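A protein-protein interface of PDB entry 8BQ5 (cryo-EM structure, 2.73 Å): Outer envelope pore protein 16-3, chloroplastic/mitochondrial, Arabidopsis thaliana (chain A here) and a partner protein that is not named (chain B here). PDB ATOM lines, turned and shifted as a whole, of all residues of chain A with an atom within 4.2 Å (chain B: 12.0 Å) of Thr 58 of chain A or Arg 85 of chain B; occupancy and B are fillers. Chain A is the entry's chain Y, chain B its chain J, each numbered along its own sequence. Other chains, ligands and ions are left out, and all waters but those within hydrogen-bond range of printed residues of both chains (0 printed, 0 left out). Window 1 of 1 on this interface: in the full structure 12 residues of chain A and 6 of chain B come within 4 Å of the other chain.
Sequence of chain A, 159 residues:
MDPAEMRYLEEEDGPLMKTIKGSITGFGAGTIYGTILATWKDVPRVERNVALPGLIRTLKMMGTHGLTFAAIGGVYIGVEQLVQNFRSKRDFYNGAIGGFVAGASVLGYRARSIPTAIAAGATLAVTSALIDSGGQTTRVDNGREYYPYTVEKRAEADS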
ATOM      1  N   ALA A  38     -18.276   5.684 -26.632  1.00  0.00           N
ATOM      2  CA  ALA A  38     -17.915   6.828 -25.805  1.00  0.00           C
ATOM      3  C   ALA A  38     -19.141   7.657 -25.447  1.00  0.00           C
ATOM      4  O   ALA A  38     -19.288   8.094 -24.301  1.00  0.00           O
ATOM      5  CB  ALA A  38     -16.873   7.682 -26.527  1.00  0.00           C
ATOM      6  N   THR A  39     -20.040   7.873 -26.411  1.00  0.00           N
ATOM      7  CA  THR A  39     -21.244   8.651 -26.138  1.00  0.00           C
ATOM      8  C   THR A  39     -22.181   7.934 -25.174  1.00  0.00           C
ATOM      9  O   THR A  39     -22.880   8.587 -24.392  1.00  0.00           O
ATOM     10  CB  THR A  39     -21.974   8.967 -27.446  1.00  0.00           C
ATOM     11  OG1 THR A  39     -21.033   9.427 -28.422  1.00  0.00           O
ATOM     12  CG2 THR A  39     -23.030  10.037 -27.227  1.00  0.00           C
ATOM     13  N   LYS A  41     -21.513   5.851 -22.579  1.00  0.00           N
ATOM     14  CA  LYS A  41     -21.083   5.890 -21.189  1.00  0.00           C
ATOM     15  C   LYS A  41     -21.199   7.298 -20.613  1.00  0.00           C
ATOM     16  O   LYS A  41     -21.163   8.302 -21.329  1.00  0.00           O
ATOM     17  CB  LYS A  41     -19.639   5.410 -21.055  1.00  0.00           C
ATOM     18  CG  LYS A  41     -19.453   3.918 -21.213  1.00  0.00           C
ATOM     19  CD  LYS A  41     -18.064   3.597 -21.742  1.00  0.00           C
ATOM     20  CE  LYS A  41     -17.814   2.101 -21.754  1.00  0.00           C
ATOM     21  NZ  LYS A  41     -16.674   1.723 -20.874  1.00  0.00           N
ATOM     22  N   VAL A  43     -19.810  10.314 -17.781  1.00  0.00           N
ATOM     23  CA  VAL A  43     -18.507  10.869 -17.428  1.00  0.00           C
ATOM     24  C   VAL A  43     -18.265  10.676 -15.937  1.00  0.00           C
ATOM     25  O   VAL A  43     -19.215  10.726 -15.140  1.00  0.00           O
ATOM     26  CB  VAL A  43     -18.397  12.351 -17.821  1.00  0.00           C
ATOM     27  CG1 VAL A  43     -18.310  12.498 -19.329  1.00  0.00           C
ATOM     28  CG2 VAL A  43     -19.585  13.122 -17.293  1.00  0.00           C
ATOM     29  N   GLY A  54     -13.366  15.056 -21.344  1.00  0.00           N
ATOM     30  CA  GLY A  54     -14.354  14.179 -21.952  1.00  0.00           C
ATOM     31  C   GLY A  54     -14.161  14.035 -23.448  1.00  0.00           C
ATOM     32  O   GLY A  54     -14.231  12.929 -23.993  1.00  0.00           O
ATOM     33  N   LEU A  55     -13.902  15.151 -24.134  1.00  0.00           N
ATOM     34  CA  LEU A  55     -13.622  15.094 -25.565  1.00  0.00           C
ATOM     35  C   LEU A  55     -12.346  14.314 -25.851  1.00  0.00           C
ATOM     36  O   LEU A  55     -12.287  13.541 -26.814  1.00  0.00           O
ATOM     37  CB  LEU A  55     -13.522  16.505 -26.140  1.00  0.00           C
ATOM     38  CG  LEU A  55     -13.244  16.571 -27.641  1.00  0.00           C
ATOM     39  CD1 LEU A  55     -14.422  16.019 -28.421  1.00  0.00           C
ATOM     40  CD2 LEU A  55     -12.931  17.994 -28.067  1.00  0.00           C
ATOM     41  N   ILE A  56     -11.306  14.519 -25.037  1.00  0.00           N
ATOM     42  CA  ILE A  56     -10.058  13.785 -25.233  1.00  0.00           C
ATOM     43  C   ILE A  56     -10.297  12.288 -25.080  1.00  0.00           C
ATOM     44  O   ILE A  56      -9.788  11.476 -25.861  1.00  0.00           O
ATOM     45  CB  ILE A  56      -8.974  14.285 -24.259  1.00  0.00           C
ATOM     46  CG1 ILE A  56      -8.794  15.802 -24.384  1.00  0.00           C
ATOM     47  CG2 ILE A  56      -7.663  13.544 -24.491  1.00  0.00           C
ATOM     48  CD1 ILE A  56      -7.681  16.230 -25.313  1.00  0.00           C
ATOM     49  N   ARG A  57     -11.079  11.902 -24.070  1.00  0.00           N
ATOM     50  CA  ARG A  57     -11.383  10.491 -23.865  1.00  0.00           C
ATOM     51  C   ARG A  57     -12.189   9.926 -25.029  1.00  0.00           C
ATOM     52  O   ARG A  57     -11.964   8.787 -25.454  1.00  0.00           O
ATOM     53  CB  ARG A  57     -12.127  10.306 -22.543  1.00  0.00           C
ATOM     54  CG  ARG A  57     -13.018   9.077 -22.485  1.00  0.00           C
ATOM     55  CD  ARG A  57     -14.003   9.153 -21.329  1.00  0.00           C
ATOM     56  NE  ARG A  57     -13.355   8.926 -20.044  1.00  0.00           N
ATOM     57  CZ  ARG A  57     -12.939   9.886 -19.230  1.00  0.00           C
ATOM     58  NH1 ARG A  57     -13.123  11.165 -19.518  1.00  0.00           N
ATOM     59  NH2 ARG A  57     -12.329   9.557 -18.095  1.00  0.00           N
ATOM     60  N   THR A  58     -13.133  10.708 -25.559  1.00  0.00           N
ATOM     61  CA  THR A  58     -13.913  10.252 -26.708  1.00  0.00           C
ATOM     62  C   THR A  58     -13.025  10.036 -27.929  1.00  0.00           C
ATOM     63  O   THR A  58     -13.139   9.019 -28.626  1.00  0.00           O
ATOM     64  CB  THR A  58     -15.019  11.259 -27.021  1.00  0.00           C
ATOM     65  OG1 THR A  58     -16.048  11.164 -26.030  1.00  0.00           O
ATOM     66  CG2 THR A  58     -15.620  10.983 -28.393  1.00  0.00           C
ATOM     67  N   LEU A  59     -12.130  10.987 -28.205  1.00  0.00           N
ATOM     68  CA  LEU A  59     -11.237  10.843 -29.350  1.00  0.00           C
ATOM     69  C   LEU A  59     -10.280   9.672 -29.154  1.00  0.00           C
ATOM     70  O   LEU A  59      -9.953   8.960 -30.112  1.00  0.00           O
ATOM     71  CB  LEU A  59     -10.470  12.144 -29.590  1.00  0.00           C
ATOM     72  CG  LEU A  59     -11.315  13.394 -29.868  1.00  0.00           C
ATOM     73  CD1 LEU A  59     -10.440  14.638 -29.903  1.00  0.00           C
ATOM     74  CD2 LEU A  59     -12.117  13.264 -31.157  1.00  0.00           C
ATOM     75  N   LYS A  60      -9.832   9.447 -27.915  1.00  0.00           N
ATOM     76  CA  LYS A  60      -8.988   8.291 -27.628  1.00  0.00           C
ATOM     77  C   LYS A  60      -9.736   6.986 -27.867  1.00  0.00           C
ATOM     78  O   LYS A  60      -9.173   6.027 -28.408  1.00  0.00           O
ATOM     79  CB  LYS A  60      -8.478   8.356 -26.188  1.00  0.00           C
ATOM     80  CG  LYS A  60      -7.222   9.194 -25.999  1.00  0.00           C
ATOM     81  CD  LYS A  60      -6.388   8.687 -24.830  1.00  0.00           C
ATOM     82  CE  LYS A  60      -6.654   9.482 -23.558  1.00  0.00           C
ATOM     83  NZ  LYS A  60      -5.877  10.753 -23.519  1.00  0.00           N
ATOM     84  N   MET A  61     -11.003   6.923 -27.451  1.00  0.00           N
ATOM     85  CA  MET A  61     -11.799   5.724 -27.690  1.00  0.00           C
ATOM     86  C   MET A  61     -11.983   5.483 -29.182  1.00  0.00           C
ATOM     87  O   MET A  61     -11.863   4.344 -29.660  1.00  0.00           O
ATOM     88  CB  MET A  61     -13.154   5.849 -26.996  1.00  0.00           C
ATOM     89  CG  MET A  61     -14.115   4.724 -27.314  1.00  0.00           C
ATOM     90  SD  MET A  61     -13.773   3.271 -26.311  1.00  0.00           S
ATOM     91  CE  MET A  61     -14.585   3.733 -24.784  1.00  0.00           C
ATOM     92  N   MET A  62     -12.261   6.550 -29.933  1.00  0.00           N
ATOM     93  CA  MET A  62     -12.376   6.428 -31.382  1.00  0.00           C
ATOM     94  C   MET A  62     -11.092   5.883 -31.986  1.00  0.00           C
ATOM     95  O   MET A  62     -11.123   4.952 -32.794  1.00  0.00           O
ATOM     96  CB  MET A  62     -12.715   7.779 -32.006  1.00  0.00           C
ATOM     97  CG  MET A  62     -14.079   8.318 -31.661  1.00  0.00           C
ATOM     98  SD  MET A  62     -14.066  10.116 -31.674  1.00  0.00           S
ATOM     99  CE  MET A  62     -14.485  10.423 -33.389  1.00  0.00           C
ATOM    100  N   ARG B  19     -29.337  24.860 -26.955  1.00  0.00           N
ATOM    101  CA  ARG B  19     -28.066  25.050 -26.269  1.00  0.00           C
ATOM    102  C   ARG B  19     -28.083  26.098 -25.167  1.00  0.00           C
ATOM    103  O   ARG B  19     -27.047  26.298 -24.524  1.00  0.00           O
ATOM    104  CB  ARG B  19     -26.962  25.428 -27.269  1.00  0.00           C
ATOM    105  CG  ARG B  19     -26.580  24.323 -28.234  1.00  0.00           C
ATOM    106  CD  ARG B  19     -25.282  23.643 -27.826  1.00  0.00           C
ATOM    107  NE  ARG B  19     -25.371  23.042 -26.500  1.00  0.00           N
ATOM    108  CZ  ARG B  19     -24.681  23.443 -25.443  1.00  0.00           C
ATOM    109  NH1 ARG B  19     -23.809  24.433 -25.520  1.00  0.00           N
ATOM    110  NH2 ARG B  19     -24.865  22.827 -24.278  1.00  0.00           N
ATOM    111  N   ILE B  79     -29.433  20.294 -14.576  1.00  0.00           N
ATOM    112  CA  ILE B  79     -29.568  20.064 -16.008  1.00  0.00           C
ATOM    113  C   ILE B  79     -28.290  20.351 -16.779  1.00  0.00           C
ATOM    114  O   ILE B  79     -28.259  20.152 -17.993  1.00  0.00           O
ATOM    115  CB  ILE B  79     -30.732  20.888 -16.595  1.00  0.00           C
ATOM    116  CG1 ILE B  79     -30.601  22.353 -16.184  1.00  0.00           C
ATOM    117  CG2 ILE B  79     -32.062  20.327 -16.135  1.00  0.00           C
ATOM    118  CD1 ILE B  79     -31.161  23.315 -17.197  1.00  0.00           C
ATOM    119  N   HIS B  80     -27.236  20.816 -16.120  1.00  0.00           N
ATOM    120  CA  HIS B  80     -26.026  21.208 -16.825  1.00  0.00           C
ATOM    121  C   HIS B  80     -25.219  19.988 -17.243  1.00  0.00           C
ATOM    122  O   HIS B  80     -25.219  18.951 -16.572  1.00  0.00           O
ATOM    123  CB  HIS B  80     -25.169  22.119 -15.946  1.00  0.00           C
ATOM    124  CG  HIS B  80     -23.810  22.404 -16.502  1.00  0.00           C
ATOM    125  ND1 HIS B  80     -23.616  23.094 -17.679  1.00  0.00           N
ATOM    126  CD2 HIS B  80     -22.575  22.108 -16.033  1.00  0.00           C
ATOM    127  CE1 HIS B  80     -22.320  23.205 -17.913  1.00  0.00           C
ATOM    128  NE2 HIS B  80     -21.667  22.615 -16.930  1.00  0.00           N
ATOM    129  N   GLU B  81     -24.523  20.124 -18.366  1.00  0.00           N
ATOM    130  CA  GLU B  81     -23.579  19.111 -18.806  1.00  0.00           C
ATOM    131  C   GLU B  81     -22.692  19.716 -19.880  1.00  0.00           C
ATOM    132  O   GLU B  81     -23.156  20.498 -20.714  1.00  0.00           O
ATOM    133  CB  GLU B  81     -24.297  17.862 -19.330  1.00  0.00           C
ATOM    134  CG  GLU B  81     -23.362  16.736 -19.703  1.00  0.00           C
ATOM    135  CD  GLU B  81     -23.745  15.433 -19.048  1.00  0.00           C
ATOM    136  OE1 GLU B  81     -23.876  15.408 -17.810  1.00  0.00           O
ATOM    137  OE2 GLU B  81     -23.902  14.429 -19.763  1.00  0.00           O
ATOM    138  N   GLU B  82     -21.413  19.359 -19.839  1.00  0.00           N
ATOM    139  CA  GLU B  82     -20.482  19.785 -20.870  1.00  0.00           C
ATOM    140  C   GLU B  82     -20.725  18.989 -22.145  1.00  0.00           C
ATOM    141  O   GLU B  82     -20.752  17.757 -22.127  1.00  0.00           O
ATOM    142  CB  GLU B  82     -19.038  19.604 -20.398  1.00  0.00           C
ATOM    143  CG  GLU B  82     -18.534  20.711 -19.484  1.00  0.00           C
ATOM    144  CD  GLU B  82     -18.643  22.091 -20.113  1.00  0.00           C
ATOM    145  OE1 GLU B  82     -18.757  23.078 -19.359  1.00  0.00           O
ATOM    146  OE2 GLU B  82     -18.610  22.190 -21.358  1.00  0.00           O
ATOM    147  N   VAL B  83     -20.903  19.703 -23.256  1.00  0.00           N
ATOM    148  CA  VAL B  83     -21.307  19.087 -24.515  1.00  0.00           C
ATOM    149  C   VAL B  83     -20.167  18.980 -25.506  1.00  0.00           C
ATOM    150  O   VAL B  83     -20.414  18.662 -26.678  1.00  0.00           O
ATOM    151  CB  VAL B  83     -22.484  19.840 -25.156  1.00  0.00           C
ATOM    152  CG1 VAL B  83     -23.705  19.781 -24.255  1.00  0.00           C
ATOM    153  CG2 VAL B  83     -22.084  21.272 -25.468  1.00  0.00           C
ATOM    154  N   LEU B  84     -18.928  19.242 -25.089  1.00  0.00           N
ATOM    155  CA  LEU B  84     -17.811  19.134 -26.022  1.00  0.00           C
ATOM    156  C   LEU B  84     -17.612  17.694 -26.471  1.00  0.00           C
ATOM    157  O   LEU B  84     -17.233  17.440 -27.620  1.00  0.00           O
ATOM    158  CB  LEU B  84     -16.537  19.681 -25.385  1.00  0.00           C
ATOM    159  CG  LEU B  84     -15.658  20.516 -26.315  1.00  0.00           C
ATOM    160  CD1 LEU B  84     -16.514  21.402 -27.203  1.00  0.00           C
ATOM    161  CD2 LEU B  84     -14.672  21.349 -25.513  1.00  0.00           C
ATOM    162  N   ARG B  85     -17.883  16.735 -25.585  1.00  0.00           N
ATOM    163  CA  ARG B  85     -17.693  15.325 -25.901  1.00  0.00           C
ATOM    164  C   ARG B  85     -18.701  14.806 -26.916  1.00  0.00           C
ATOM    165  O   ARG B  85     -18.558  13.668 -27.375  1.00  0.00           O
ATOM    166  CB  ARG B  85     -17.774  14.486 -24.626  1.00  0.00           C
ATOM    167  CG  ARG B  85     -19.142  14.475 -23.972  1.00  0.00           C
ATOM    168  CD  ARG B  85     -19.154  13.562 -22.761  1.00  0.00           C
ATOM    169  NE  ARG B  85     -19.143  12.156 -23.145  1.00  0.00           N
ATOM    170  CZ  ARG B  85     -19.944  11.231 -22.637  1.00  0.00           C
ATOM    171  NH1 ARG B  85     -20.840  11.525 -21.711  1.00  0.00           N
ATOM    172  NH2 ARG B  85     -19.840   9.977 -23.065  1.00  0.00           N
ATOM    173  N   TYR B  86     -19.721  15.589 -27.257  1.00  0.00           N
ATOM    174  CA  TYR B  86     -20.718  15.164 -28.226  1.00  0.00           C
ATOM    175  C   TYR B  86     -20.466  15.716 -29.619  1.00  0.00           C
ATOM    176  O   TYR B  86     -21.260  15.447 -30.524  1.00  0.00           O
ATOM    177  CB  TYR B  86     -22.113  15.567 -27.747  1.00  0.00           C
ATOM    178  CG  TYR B  86     -22.477  14.881 -26.458  1.00  0.00           C
ATOM    179  CD1 TYR B  86     -22.924  13.569 -26.455  1.00  0.00           C
ATOM    180  CD2 TYR B  86     -22.337  15.530 -25.243  1.00  0.00           C
ATOM    181  CE1 TYR B  86     -23.240  12.931 -25.278  1.00  0.00           C
ATOM    182  CE2 TYR B  86     -22.651  14.900 -24.061  1.00  0.00           C
ATOM    183  CZ  TYR B  86     -23.100  13.600 -24.086  1.00  0.00           C
ATOM    184  OH  TYR B  86     -23.411  12.963 -22.914  1.00  0.00           O
ATOM    185  N   LEU B  87     -19.390  16.476 -29.808  1.00  0.00           N
ATOM    186  CA  LEU B  87     -19.032  16.947 -31.142  1.00  0.00           C
ATOM    187  C   LEU B  87     -18.840  15.817 -32.149  1.00  0.00           C
ATOM    188  O   LEU B  87     -19.393  15.919 -33.257  1.00  0.00           O
ATOM    189  CB  LEU B  87     -17.771  17.825 -31.054  1.00  0.00           C
ATOM    190  CG  LEU B  87     -17.621  19.039 -31.983  1.00  0.00           C
ATOM    191  CD1 LEU B  87     -18.374  20.230 -31.469  1.00  0.00           C
ATOM    192  CD2 LEU B  87     -16.165  19.427 -32.178  1.00  0.00           C
ATOM    193  N   PRO B  88     -18.103  14.723 -31.851  1.00  0.00           N
ATOM    194  CA  PRO B  88     -17.931  13.668 -32.863  1.00  0.00           C
ATOM    195  C   PRO B  88     -19.215  12.935 -33.222  1.00  0.00           C
ATOM    196  O   PRO B  88     -19.500  12.756 -34.408  1.00  0.00           O
ATOM    197  CB  PRO B  88     -16.916  12.715 -32.220  1.00  0.00           C
ATOM    198  CG  PRO B  88     -16.302  13.460 -31.108  1.00  0.00           C
ATOM    199  CD  PRO B  88     -17.297  14.459 -30.645  1.00  0.00           C
ATOM    200  N   VAL B  89     -19.987  12.489 -32.228  1.00  0.00           N
ATOM    201  CA  VAL B  89     -21.210  11.748 -32.533  1.00  0.00           C
ATOM    202  C   VAL B  89     -22.217  12.647 -33.240  1.00  0.00           C
ATOM    203  O   VAL B  89     -22.867  12.235 -34.211  1.00  0.00           O
ATOM    204  CB  VAL B  89     -21.799  11.105 -31.258  1.00  0.00           C
ATOM    205  CG1 VAL B  89     -22.345  12.153 -30.291  1.00  0.00           C
ATOM    206  CG2 VAL B  89     -22.874  10.094 -31.626  1.00  0.00           C
ATOM    207  N   SER B  90     -22.357  13.890 -32.771  1.00  0.00           N
ATOM    208  CA  SER B  90     -23.226  14.834 -33.458  1.00  0.00           C
ATOM    209  C   SER B  90     -22.688  15.160 -34.838  1.00  0.00           C
ATOM    210  O   SER B  90     -23.468  15.304 -35.779  1.00  0.00           O
ATOM    211  CB  SER B  90     -23.396  16.111 -32.636  1.00  0.00           C
ATOM    212  OG  SER B  90     -22.172  16.814 -32.516  1.00  0.00           O
ATOM    213  N   GLY B  91     -21.367  15.258 -34.985  1.00  0.00           N
ATOM    214  CA  GLY B  91     -20.803  15.467 -36.308  1.00  0.00           C
ATOM    215  C   GLY B  91     -21.174  14.356 -37.272  1.00  0.00           C
ATOM    216  O   GLY B  91     -21.642  14.615 -38.381  1.00  0.00           O
ATOM    217  N   ILE B  92     -21.008  13.102 -36.842  1.00  0.00           N
ATOM    218  CA  ILE B  92     -21.307  11.964 -37.708  1.00  0.00           C
ATOM    219  C   ILE B  92     -22.790  11.933 -38.058  1.00  0.00           C
ATOM    220  O   ILE B  92     -23.165  11.855 -39.237  1.00  0.00           O
ATOM    221  CB  ILE B  92     -20.860  10.652 -37.039  1.00  0.00           C
ATOM    222  CG1 ILE B  92     -19.402  10.340 -37.374  1.00  0.00           C
ATOM    223  CG2 ILE B  92     -21.746   9.491 -37.467  1.00  0.00           C
ATOM    224  CD1 ILE B  92     -18.717   9.483 -36.334  1.00  0.00           C
ATOM    225  N   ILE B  93     -23.656  12.008 -37.043  1.00  0.00           N
ATOM    226  CA  ILE B  93     -25.089  11.892 -37.294  1.00  0.00           C
ATOM    227  C   ILE B  93     -25.571  13.059 -38.147  1.00  0.00           C
ATOM    228  O   ILE B  93     -26.340  12.875 -39.101  1.00  0.00           O
ATOM    229  CB  ILE B  93     -25.863  11.796 -35.965  1.00  0.00           C
ATOM    230  CG1 ILE B  93     -25.450  10.543 -35.184  1.00  0.00           C
ATOM    231  CG2 ILE B  93     -27.358  11.771 -36.223  1.00  0.00           C
ATOM    232  CD1 ILE B  93     -25.934   9.247 -35.790  1.00  0.00           C
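NH2 of Arg 85 of chain B lies within hydrogen-bond range of O of Lys 41 of chain A (2.8 Å). The guanidinium group of Arg 85 of chain B lies close to the backbone carbonyl oxygen of Ala 38 of chain A (2.3 Å).
OH of Tyr 86 of chain B is in hydrogen-bond range of NH1 of Arg 85 of chain B (3.2 Å). The side-chain hydroxyl (OG) of Ser 90 of chain B lies within hydrogen-bond range of the backbone carbonyl oxygen (O) of Tyr 86 of chain B (2.6 Å). O of Gly 54 of chain A sits at hydrogen-bond distance from OG1 of Thr 58 of chain A, 3.3 Å away.
Thr 39 of chain A touches Arg 85 of chain B (O to NH2, 3.6 Å). Tyr 86 of chain B touches Thr 39 of chain A. Thr 39 of chain A touches Val 89 of chain B. Val 43 of chain A touches Arg 85 of chain B. Gly 54 of chain A touches Arg 85 of chain B. Leu 84 of chain B touches Leu 55 of chain A (O to CD1, 3.3 Å). Arg 85 of chain B touches Leu 55 of chain A. Thr 58 of chain A touches Arg 85 of chain B (OG1 to O, 3.8 Å). Thr 58 of chain A touches Pro 88 of chain B (CG2 to CG, 3.7 Å). CB of Pro 88 of chain B touches CE of Met 62 of chain A (3.5 Å).
Of chain B, only Arg 85 (2.3 Å) comes within 4 Å of Ala 38 of chain A. Thr 39 of chain A touches just these residues of chain B: Arg 85, Tyr 86 and Val 89. Of the printed residues of chain B, Lys 41 of chain A touches Arg 85. Gly 54 of chain A touches just one residue of chain B: Arg 85 (3.8 Å). Leu 55 of chain A touches three residues of chain B. No residue of chain B comes within 4 Å of Ile 56 of chain A. Thr 58 of chain A touches two residues of chain B. No residue of chain B comes within 4 Å of Leu 59 of chain A. Lys 60 of chain A touches none of the printed residues of chain B. Of the printed residues of chain B, Met 62 of chain A touches Pro 88 (3.5 Å). Printed residues of chain A within 4 Å of Leu 84 of chain B: Leu 55 (3.3 Å). Of chain A, only Ala 38, Thr 39, Lys 41, Val 43, Gly 54, Leu 55 and Thr 58 come within 4 Å of Arg 85 of chain B. Of the printed residues of chain A, Tyr 86 of chain B touches Thr 39. The nearest residue of chain B that does not touch Thr 58 of chain A is Tyr 86 of chain B (5.9 Å). The nearest printed residue of chain A that does not touch Arg 85 of chain B is Arg 57 of chain A (6.1 Å). The nearest printed residue of chain A that does not touch Val 89 of chain B is Met 62 of chain A (6.0 Å).
Of the 13 printed residues of chain A, 8 touch a printed residue of chain B. Hydrophobic or aromatic side chains of chain A that line the printed part of chain B: Val 43, Leu 55 and Met 62. Along chain A the printed residues that touch a printed residue of chain B span positions 38 to 62. Of the 16 printed residues of chain B, 5 touch a printed residue of chain A. Hydrophobic or aromatic side chains of chain B that line the printed part of chain A: Tyr 86, Pro 88 and Val 89.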
